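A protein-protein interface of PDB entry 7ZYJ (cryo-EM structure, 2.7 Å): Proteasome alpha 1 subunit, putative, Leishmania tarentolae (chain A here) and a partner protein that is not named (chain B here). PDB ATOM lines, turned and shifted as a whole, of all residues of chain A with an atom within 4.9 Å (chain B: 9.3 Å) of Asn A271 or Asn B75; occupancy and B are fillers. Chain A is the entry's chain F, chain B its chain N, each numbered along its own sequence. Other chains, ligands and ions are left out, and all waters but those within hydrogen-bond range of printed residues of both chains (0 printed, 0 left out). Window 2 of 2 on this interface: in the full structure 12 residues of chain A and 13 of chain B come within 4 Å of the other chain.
A ring nitrogen (ND1) of His B74 lies within hydrogen-bond range of the side-chain carboxylate (OD2) of Asp A275, 3.0 Å away.
The side-chain amide nitrogen of Gln A305 is in hydrogen-bond range of the backbone carbonyl oxygen of Asn B75, at 2.9 Å.
The backbone carbonyl oxygen (O) of Asn B75 lies within hydrogen-bond range of the side-chain amide nitrogen (ND2) of Asn A271 (2.8 Å).
The side-chain amide nitrogen (NE2) of Gln B70 is in hydrogen-bond range of the side-chain amide oxygen (OE1) of Gln A272 (3.1 Å).
OD1 of Asp A303 lies close to N of Gln A305 (3.4 Å).
The side-chain amide oxygen (OD1) of Asn A271 is in hydrogen-bond range of the side-chain hydroxyl (OH) of Tyr A310.
The side-chain amide oxygen of Gln A305 is in hydrogen-bond range of the side-chain amide nitrogen of Asn A271 (3.1 Å).
Val B76 touches Pro A269 (CG1 to CB, 3.6 Å).
Asn A271 touches Val B76.
CG of Gln A272 touches NE2 of His B74, at 3.7 Å.
Val B76 touches Gln A305.
Of the printed residues of chain B, Pro A269 touches Val B76.
Of the printed residues of chain B, Asn A271 touches Asn B75 (2.8 Å) and Val B76 (3.997 Å).
No residue of chain B comes within 4 Å of Ala A274.
Of the printed residues of chain B, Asp A275 touches His B74 (3.0 Å).
Printed residues of chain A within 4 Å of His B74: Gln A272 (3.7 Å) and Asp A275 (3.0 Å).
Printed residues of chain A within 4 Å of Asn B75: Asn A271 and Gln A305.
The nearest printed residue of chain B that does not touch Asn A271 is His B74 (4.7 Å).
The nearest printed residue of chain A that does not touch Asn B75 is Asp A275 (5.2 Å).
The nearest printed residue of chain B that does not touch Pro A269 is Gln B70 (4.3 Å).
Of the 10 printed residues of chain B, 4 touch a printed residue of chain A.
Hydrophobic or aromatic side chains of chain B that line the printed part of chain A: His B74 and Val B76.
Hydrophobic or aromatic side chains of chain A within 4 Å of the printed part of chain B: Pro A269.
Among the printed residues, no Asp or Glu carboxylate lies within 4 Å of a Lys or Arg side-chain nitrogen of the other chain.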
ATOM      1  N   PRO A 269       8.581  -6.832  -7.951  1.00  0.00           N
ATOM      2  CA  PRO A 269       9.805  -6.367  -7.290  1.00  0.00           C
ATOM      3  C   PRO A 269      10.901  -6.079  -8.302  1.00  0.00           C
ATOM      4  O   PRO A 269      10.978  -6.695  -9.368  1.00  0.00           O
ATOM      5  CB  PRO A 269      10.185  -7.534  -6.371  1.00  0.00           C
ATOM      6  CG  PRO A 269       8.959  -8.386  -6.280  1.00  0.00           C
ATOM      7  CD  PRO A 269       8.233  -8.209  -7.569  1.00  0.00           C
ATOM      8  N   MET A 270      11.762  -5.122  -7.950  1.00  0.00           N
ATOM      9  CA  MET A 270      12.741  -4.619  -8.908  1.00  0.00           C
ATOM     10  C   MET A 270      13.837  -5.638  -9.194  1.00  0.00           C
ATOM     11  O   MET A 270      14.344  -5.705 -10.318  1.00  0.00           O
ATOM     12  CB  MET A 270      13.339  -3.308  -8.404  1.00  0.00           C
ATOM     13  CG  MET A 270      12.337  -2.173  -8.356  1.00  0.00           C
ATOM     14  SD  MET A 270      11.839  -1.657 -10.008  1.00  0.00           S
ATOM     15  CE  MET A 270      13.423  -1.235 -10.728  1.00  0.00           C
ATOM     16  N   ASN A 271      14.233  -6.427  -8.191  1.00  0.00           N
ATOM     17  CA  ASN A 271      15.256  -7.443  -8.422  1.00  0.00           C
ATOM     18  C   ASN A 271      14.774  -8.501  -9.407  1.00  0.00           C
ATOM     19  O   ASN A 271      15.505  -8.887 -10.329  1.00  0.00           O
ATOM     20  CB  ASN A 271      15.665  -8.087  -7.098  1.00  0.00           C
ATOM     21  CG  ASN A 271      16.436  -7.139  -6.201  1.00  0.00           C
ATOM     22  OD1 ASN A 271      17.528  -6.690  -6.546  1.00  0.00           O
ATOM     23  ND2 ASN A 271      15.869  -6.829  -5.042  1.00  0.00           N
ATOM     24  N   GLN A 272      13.538  -8.976  -9.232  1.00  0.00           N
ATOM     25  CA  GLN A 272      12.965  -9.930 -10.173  1.00  0.00           C
ATOM     26  C   GLN A 272      12.864  -9.327 -11.567  1.00  0.00           C
ATOM     27  O   GLN A 272      13.131 -10.004 -12.567  1.00  0.00           O
ATOM     28  CB  GLN A 272      11.591 -10.383  -9.683  1.00  0.00           C
ATOM     29  CG  GLN A 272      10.937 -11.445 -10.545  1.00  0.00           C
ATOM     30  CD  GLN A 272       9.601 -11.895  -9.994  1.00  0.00           C
ATOM     31  OE1 GLN A 272       9.208 -11.506  -8.896  1.00  0.00           O
ATOM     32  NE2 GLN A 272       8.895 -12.721 -10.755  1.00  0.00           N
ATOM     33  N   MET A 273      12.487  -8.050 -11.648  1.00  0.00           N
ATOM     34  CA  MET A 273      12.408  -7.379 -12.939  1.00  0.00           C
ATOM     35  C   MET A 273      13.768  -7.323 -13.618  1.00  0.00           C
ATOM     36  O   MET A 273      13.879  -7.597 -14.816  1.00  0.00           O
ATOM     37  CB  MET A 273      11.858  -5.971 -12.753  1.00  0.00           C
ATOM     38  CG  MET A 273      11.620  -5.226 -14.042  1.00  0.00           C
ATOM     39  SD  MET A 273      10.969  -3.596 -13.682  1.00  0.00           S
ATOM     40  CE  MET A 273       9.329  -4.043 -13.142  1.00  0.00           C
ATOM     41  N   ALA A 274      14.812  -6.961 -12.868  1.00  0.00           N
ATOM     42  CA  ALA A 274      16.153  -6.899 -13.436  1.00  0.00           C
ATOM     43  C   ALA A 274      16.607  -8.269 -13.915  1.00  0.00           C
ATOM     44  O   ALA A 274      17.226  -8.392 -14.980  1.00  0.00           O
ATOM     45  CB  ALA A 274      17.132  -6.333 -12.409  1.00  0.00           C
ATOM     46  N   ASP A 275      16.305  -9.314 -13.141  1.00  0.00           N
ATOM     47  CA  ASP A 275      16.627 -10.667 -13.581  1.00  0.00           C
ATOM     48  C   ASP A 275      15.903 -11.009 -14.878  1.00  0.00           C
ATOM     49  O   ASP A 275      16.479 -11.645 -15.769  1.00  0.00           O
ATOM     50  CB  ASP A 275      16.279 -11.676 -12.487  1.00  0.00           C
ATOM     51  CG  ASP A 275      17.112 -11.490 -11.236  1.00  0.00           C
ATOM     52  OD1 ASP A 275      18.346 -11.350 -11.358  1.00  0.00           O
ATOM     53  OD2 ASP A 275      16.535 -11.491 -10.128  1.00  0.00           O
ATOM     54  N   ASP A 303       9.919  -0.338  -4.516  1.00  0.00           N
ATOM     55  CA  ASP A 303       9.150  -1.465  -4.002  1.00  0.00           C
ATOM     56  C   ASP A 303       9.302  -1.485  -2.484  1.00  0.00           C
ATOM     57  O   ASP A 303       9.705  -0.488  -1.877  1.00  0.00           O
ATOM     58  CB  ASP A 303       9.597  -2.775  -4.674  1.00  0.00           C
ATOM     59  CG  ASP A 303      11.091  -3.000  -4.575  1.00  0.00           C
ATOM     60  OD1 ASP A 303      11.798  -2.083  -4.111  1.00  0.00           O
ATOM     61  OD2 ASP A 303      11.559  -4.091  -4.961  1.00  0.00           O
ATOM     62  N   GLN A 305      11.507  -2.928  -0.835  1.00  0.00           N
ATOM     63  CA  GLN A 305      12.921  -2.855  -0.493  1.00  0.00           C
ATOM     64  C   GLN A 305      13.512  -1.467  -0.701  1.00  0.00           C
ATOM     65  O   GLN A 305      14.703  -1.273  -0.438  1.00  0.00           O
ATOM     66  CB  GLN A 305      13.708  -3.884  -1.305  1.00  0.00           C
ATOM     67  CG  GLN A 305      13.560  -5.306  -0.798  1.00  0.00           C
ATOM     68  CD  GLN A 305      14.000  -6.338  -1.814  1.00  0.00           C
ATOM     69  OE1 GLN A 305      13.641  -6.263  -2.988  1.00  0.00           O
ATOM     70  NE2 GLN A 305      14.784  -7.312  -1.366  1.00  0.00           N
ATOM     71  N   HIS A 308      15.425   1.688  -6.314  1.00  0.00           N
ATOM     72  CA  HIS A 308      16.306   0.840  -7.103  1.00  0.00           C
ATOM     73  C   HIS A 308      16.687   1.555  -8.390  1.00  0.00           C
ATOM     74  O   HIS A 308      15.884   2.302  -8.956  1.00  0.00           O
ATOM     75  CB  HIS A 308      15.644  -0.504  -7.426  1.00  0.00           C
ATOM     76  CG  HIS A 308      15.562  -1.431  -6.254  1.00  0.00           C
ATOM     77  ND1 HIS A 308      14.552  -1.364  -5.318  1.00  0.00           N
ATOM     78  CD2 HIS A 308      16.366  -2.449  -5.866  1.00  0.00           C
ATOM     79  CE1 HIS A 308      14.739  -2.298  -4.404  1.00  0.00           C
ATOM     80  NE2 HIS A 308      15.832  -2.971  -4.713  1.00  0.00           N
ATOM     81  N   TYR A 310      18.860   0.391 -11.923  1.00  0.00           N
ATOM     82  CA  TYR A 310      19.565  -0.646 -12.658  1.00  0.00           C
ATOM     83  C   TYR A 310      20.011  -0.134 -14.019  1.00  0.00           C
ATOM     84  O   TYR A 310      19.427   0.793 -14.585  1.00  0.00           O
ATOM     85  CB  TYR A 310      18.685  -1.886 -12.839  1.00  0.00           C
ATOM     86  CG  TYR A 310      18.346  -2.595 -11.551  1.00  0.00           C
ATOM     87  CD1 TYR A 310      19.158  -3.608 -11.062  1.00  0.00           C
ATOM     88  CD2 TYR A 310      17.212  -2.257 -10.828  1.00  0.00           C
ATOM     89  CE1 TYR A 310      18.853  -4.261  -9.887  1.00  0.00           C
ATOM     90  CE2 TYR A 310      16.899  -2.906  -9.652  1.00  0.00           C
ATOM     91  CZ  TYR A 310      17.722  -3.906  -9.186  1.00  0.00           C
ATOM     92  OH  TYR A 310      17.413  -4.554  -8.013  1.00  0.00           O
ATOM     93  N   ARG B  69       9.997 -20.572  -4.492  1.00  0.00           N
ATOM     94  CA  ARG B  69      10.858 -20.349  -5.649  1.00  0.00           C
ATOM     95  C   ARG B  69      11.072 -18.863  -5.904  1.00  0.00           C
ATOM     96  O   ARG B  69      12.185 -18.439  -6.228  1.00  0.00           O
ATOM     97  CB  ARG B  69      10.266 -21.034  -6.880  1.00  0.00           C
ATOM     98  CG  ARG B  69      10.530 -22.527  -6.919  1.00  0.00           C
ATOM     99  CD  ARG B  69       9.578 -23.240  -7.856  1.00  0.00           C
ATOM    100  NE  ARG B  69       9.491 -24.664  -7.550  1.00  0.00           N
ATOM    101  CZ  ARG B  69       8.746 -25.529  -8.224  1.00  0.00           C
ATOM    102  NH1 ARG B  69       8.013 -25.153  -9.258  1.00  0.00           N
ATOM    103  NH2 ARG B  69       8.738 -26.806  -7.851  1.00  0.00           N
ATOM    104  N   GLN B  70      10.018 -18.055  -5.762  1.00  0.00           N
ATOM    105  CA  GLN B  70      10.173 -16.614  -5.931  1.00  0.00           C
ATOM    106  C   GLN B  70      11.081 -16.025  -4.861  1.00  0.00           C
ATOM    107  O   GLN B  70      11.918 -15.163  -5.152  1.00  0.00           O
ATOM    108  CB  GLN B  70       8.811 -15.923  -5.910  1.00  0.00           C
ATOM    109  CG  GLN B  70       8.892 -14.429  -6.167  1.00  0.00           C
ATOM    110  CD  GLN B  70       7.533 -13.766  -6.202  1.00  0.00           C
ATOM    111  OE1 GLN B  70       6.508 -14.415  -5.997  1.00  0.00           O
ATOM    112  NE2 GLN B  70       7.518 -12.463  -6.457  1.00  0.00           N
ATOM    113  N   LYS B  71      10.926 -16.469  -3.611  1.00  0.00           N
ATOM    114  CA  LYS B  71      11.794 -15.973  -2.549  1.00  0.00           C
ATOM    115  C   LYS B  71      13.244 -16.391  -2.762  1.00  0.00           C
ATOM    116  O   LYS B  71      14.161 -15.616  -2.472  1.00  0.00           O
ATOM    117  CB  LYS B  71      11.295 -16.463  -1.190  1.00  0.00           C
ATOM    118  CG  LYS B  71      12.113 -15.962  -0.012  1.00  0.00           C
ATOM    119  CD  LYS B  71      11.492 -16.376   1.311  1.00  0.00           C
ATOM    120  CE  LYS B  71      11.686 -17.860   1.570  1.00  0.00           C
ATOM    121  NZ  LYS B  71      11.188 -18.261   2.914  1.00  0.00           N
ATOM    122  N   MET B  72      13.469 -17.604  -3.267  1.00  0.00           N
ATOM    123  CA  MET B  72      14.807 -18.162  -3.414  1.00  0.00           C
ATOM    124  C   MET B  72      15.523 -17.676  -4.668  1.00  0.00           C
ATOM    125  O   MET B  72      16.724 -17.386  -4.620  1.00  0.00           O
ATOM    126  CB  MET B  72      14.730 -19.691  -3.431  1.00  0.00           C
ATOM    127  CG  MET B  72      16.022 -20.388  -3.056  1.00  0.00           C
ATOM    128  SD  MET B  72      16.201 -21.972  -3.898  1.00  0.00           S
ATOM    129  CE  MET B  72      14.710 -22.807  -3.367  1.00  0.00           C
ATOM    130  N   TYR B  73      14.814 -17.584  -5.794  1.00  0.00           N
ATOM    131  CA  TYR B  73      15.467 -17.258  -7.057  1.00  0.00           C
ATOM    132  C   TYR B  73      15.878 -15.792  -7.124  1.00  0.00           C
ATOM    133  O   TYR B  73      16.915 -15.464  -7.711  1.00  0.00           O
ATOM    134  CB  TYR B  73      14.550 -17.607  -8.230  1.00  0.00           C
ATOM    135  CG  TYR B  73      14.290 -19.087  -8.406  1.00  0.00           C
ATOM    136  CD1 TYR B  73      14.957 -20.031  -7.635  1.00  0.00           C
ATOM    137  CD2 TYR B  73      13.374 -19.541  -9.344  1.00  0.00           C
ATOM    138  CE1 TYR B  73      14.718 -21.381  -7.793  1.00  0.00           C
ATOM    139  CE2 TYR B  73      13.129 -20.889  -9.510  1.00  0.00           C
ATOM    140  CZ  TYR B  73      13.803 -21.804  -8.732  1.00  0.00           C
ATOM    141  OH  TYR B  73      13.562 -23.148  -8.894  1.00  0.00           O
ATOM    142  N   HIS B  74      15.086 -14.901  -6.539  1.00  0.00           N
ATOM    143  CA  HIS B  74      15.366 -13.475  -6.558  1.00  0.00           C
ATOM    144  C   HIS B  74      15.445 -12.932  -5.139  1.00  0.00           C
ATOM    145  O   HIS B  74      14.760 -13.413  -4.232  1.00  0.00           O
ATOM    146  CB  HIS B  74      14.297 -12.714  -7.346  1.00  0.00           C
ATOM    147  CG  HIS B  74      13.737 -13.483  -8.500  1.00  0.00           C
ATOM    148  ND1 HIS B  74      14.410 -13.631  -9.694  1.00  0.00           N
ATOM    149  CD2 HIS B  74      12.568 -14.151  -8.644  1.00  0.00           C
ATOM    150  CE1 HIS B  74      13.681 -14.354 -10.523  1.00  0.00           C
ATOM    151  NE2 HIS B  74      12.558 -14.684  -9.910  1.00  0.00           N
ATOM    152  N   ASN B  75      16.293 -11.920  -4.955  1.00  0.00           N
ATOM    153  CA  ASN B  75      16.472 -11.283  -3.650  1.00  0.00           C
ATOM    154  C   ASN B  75      15.301 -10.332  -3.424  1.00  0.00           C
ATOM    155  O   ASN B  75      15.415  -9.106  -3.517  1.00  0.00           O
ATOM    156  CB  ASN B  75      17.814 -10.565  -3.582  1.00  0.00           C
ATOM    157  CG  ASN B  75      18.031  -9.862  -2.257  1.00  0.00           C
ATOM    158  OD1 ASN B  75      17.853 -10.453  -1.193  1.00  0.00           O
ATOM    159  ND2 ASN B  75      18.423  -8.595  -2.317  1.00  0.00           N
ATOM    160  N   VAL B  76      14.143 -10.920  -3.127  1.00  0.00           N
ATOM    161  CA  VAL B  76      12.908 -10.174  -2.950  1.00  0.00           C
ATOM    162  C   VAL B  76      12.263 -10.594  -1.638  1.00  0.00           C
ATOM    163  O   VAL B  76      12.550 -11.658  -1.087  1.00  0.00           O
ATOM    164  CB  VAL B  76      11.924 -10.388  -4.121  1.00  0.00           C
ATOM    165  CG1 VAL B  76      12.571  -9.998  -5.439  1.00  0.00           C
ATOM    166  CG2 VAL B  76      11.451 -11.831  -4.161  1.00  0.00           C
ATOM    167  N   ASP B  77      11.385  -9.731  -1.137  1.00  0.00           N
ATOM    168  CA  ASP B  77      10.622 -10.058   0.055  1.00  0.00           C
ATOM    169  C   ASP B  77       9.635 -11.183  -0.238  1.00  0.00           C
ATOM    170  O   ASP B  77       9.177 -11.370  -1.369  1.00  0.00           O
ATOM    171  CB  ASP B  77       9.877  -8.830   0.574  1.00  0.00           C
ATOM    172  CG  ASP B  77      10.785  -7.862   1.301  1.00  0.00           C
ATOM    173  OD1 ASP B  77      11.846  -8.296   1.795  1.00  0.00           O
ATOM    174  OD2 ASP B  77      10.438  -6.665   1.381  1.00  0.00           O
ATOM    175  N   GLU B  78       9.317 -11.946   0.803  1.00  0.00           N
ATOM    176  CA  GLU B  78       8.337 -13.012   0.673  1.00  0.00           C
ATOM    177  C   GLU B  78       6.962 -12.428   0.369  1.00  0.00           C
ATOM    178  O   GLU B  78       6.618 -11.329   0.811  1.00  0.00           O
ATOM    179  CB  GLU B  78       8.296 -13.846   1.952  1.00  0.00           C
ATOM    180  CG  GLU B  78       7.410 -15.073   1.883  1.00  0.00           C
ATOM    181  CD  GLU B  78       7.428 -15.868   3.169  1.00  0.00           C
ATOM    182  OE1 GLU B  78       8.197 -15.504   4.084  1.00  0.00           O
ATOM    183  OE2 GLU B  78       6.674 -16.854   3.270  1.00  0.00           O
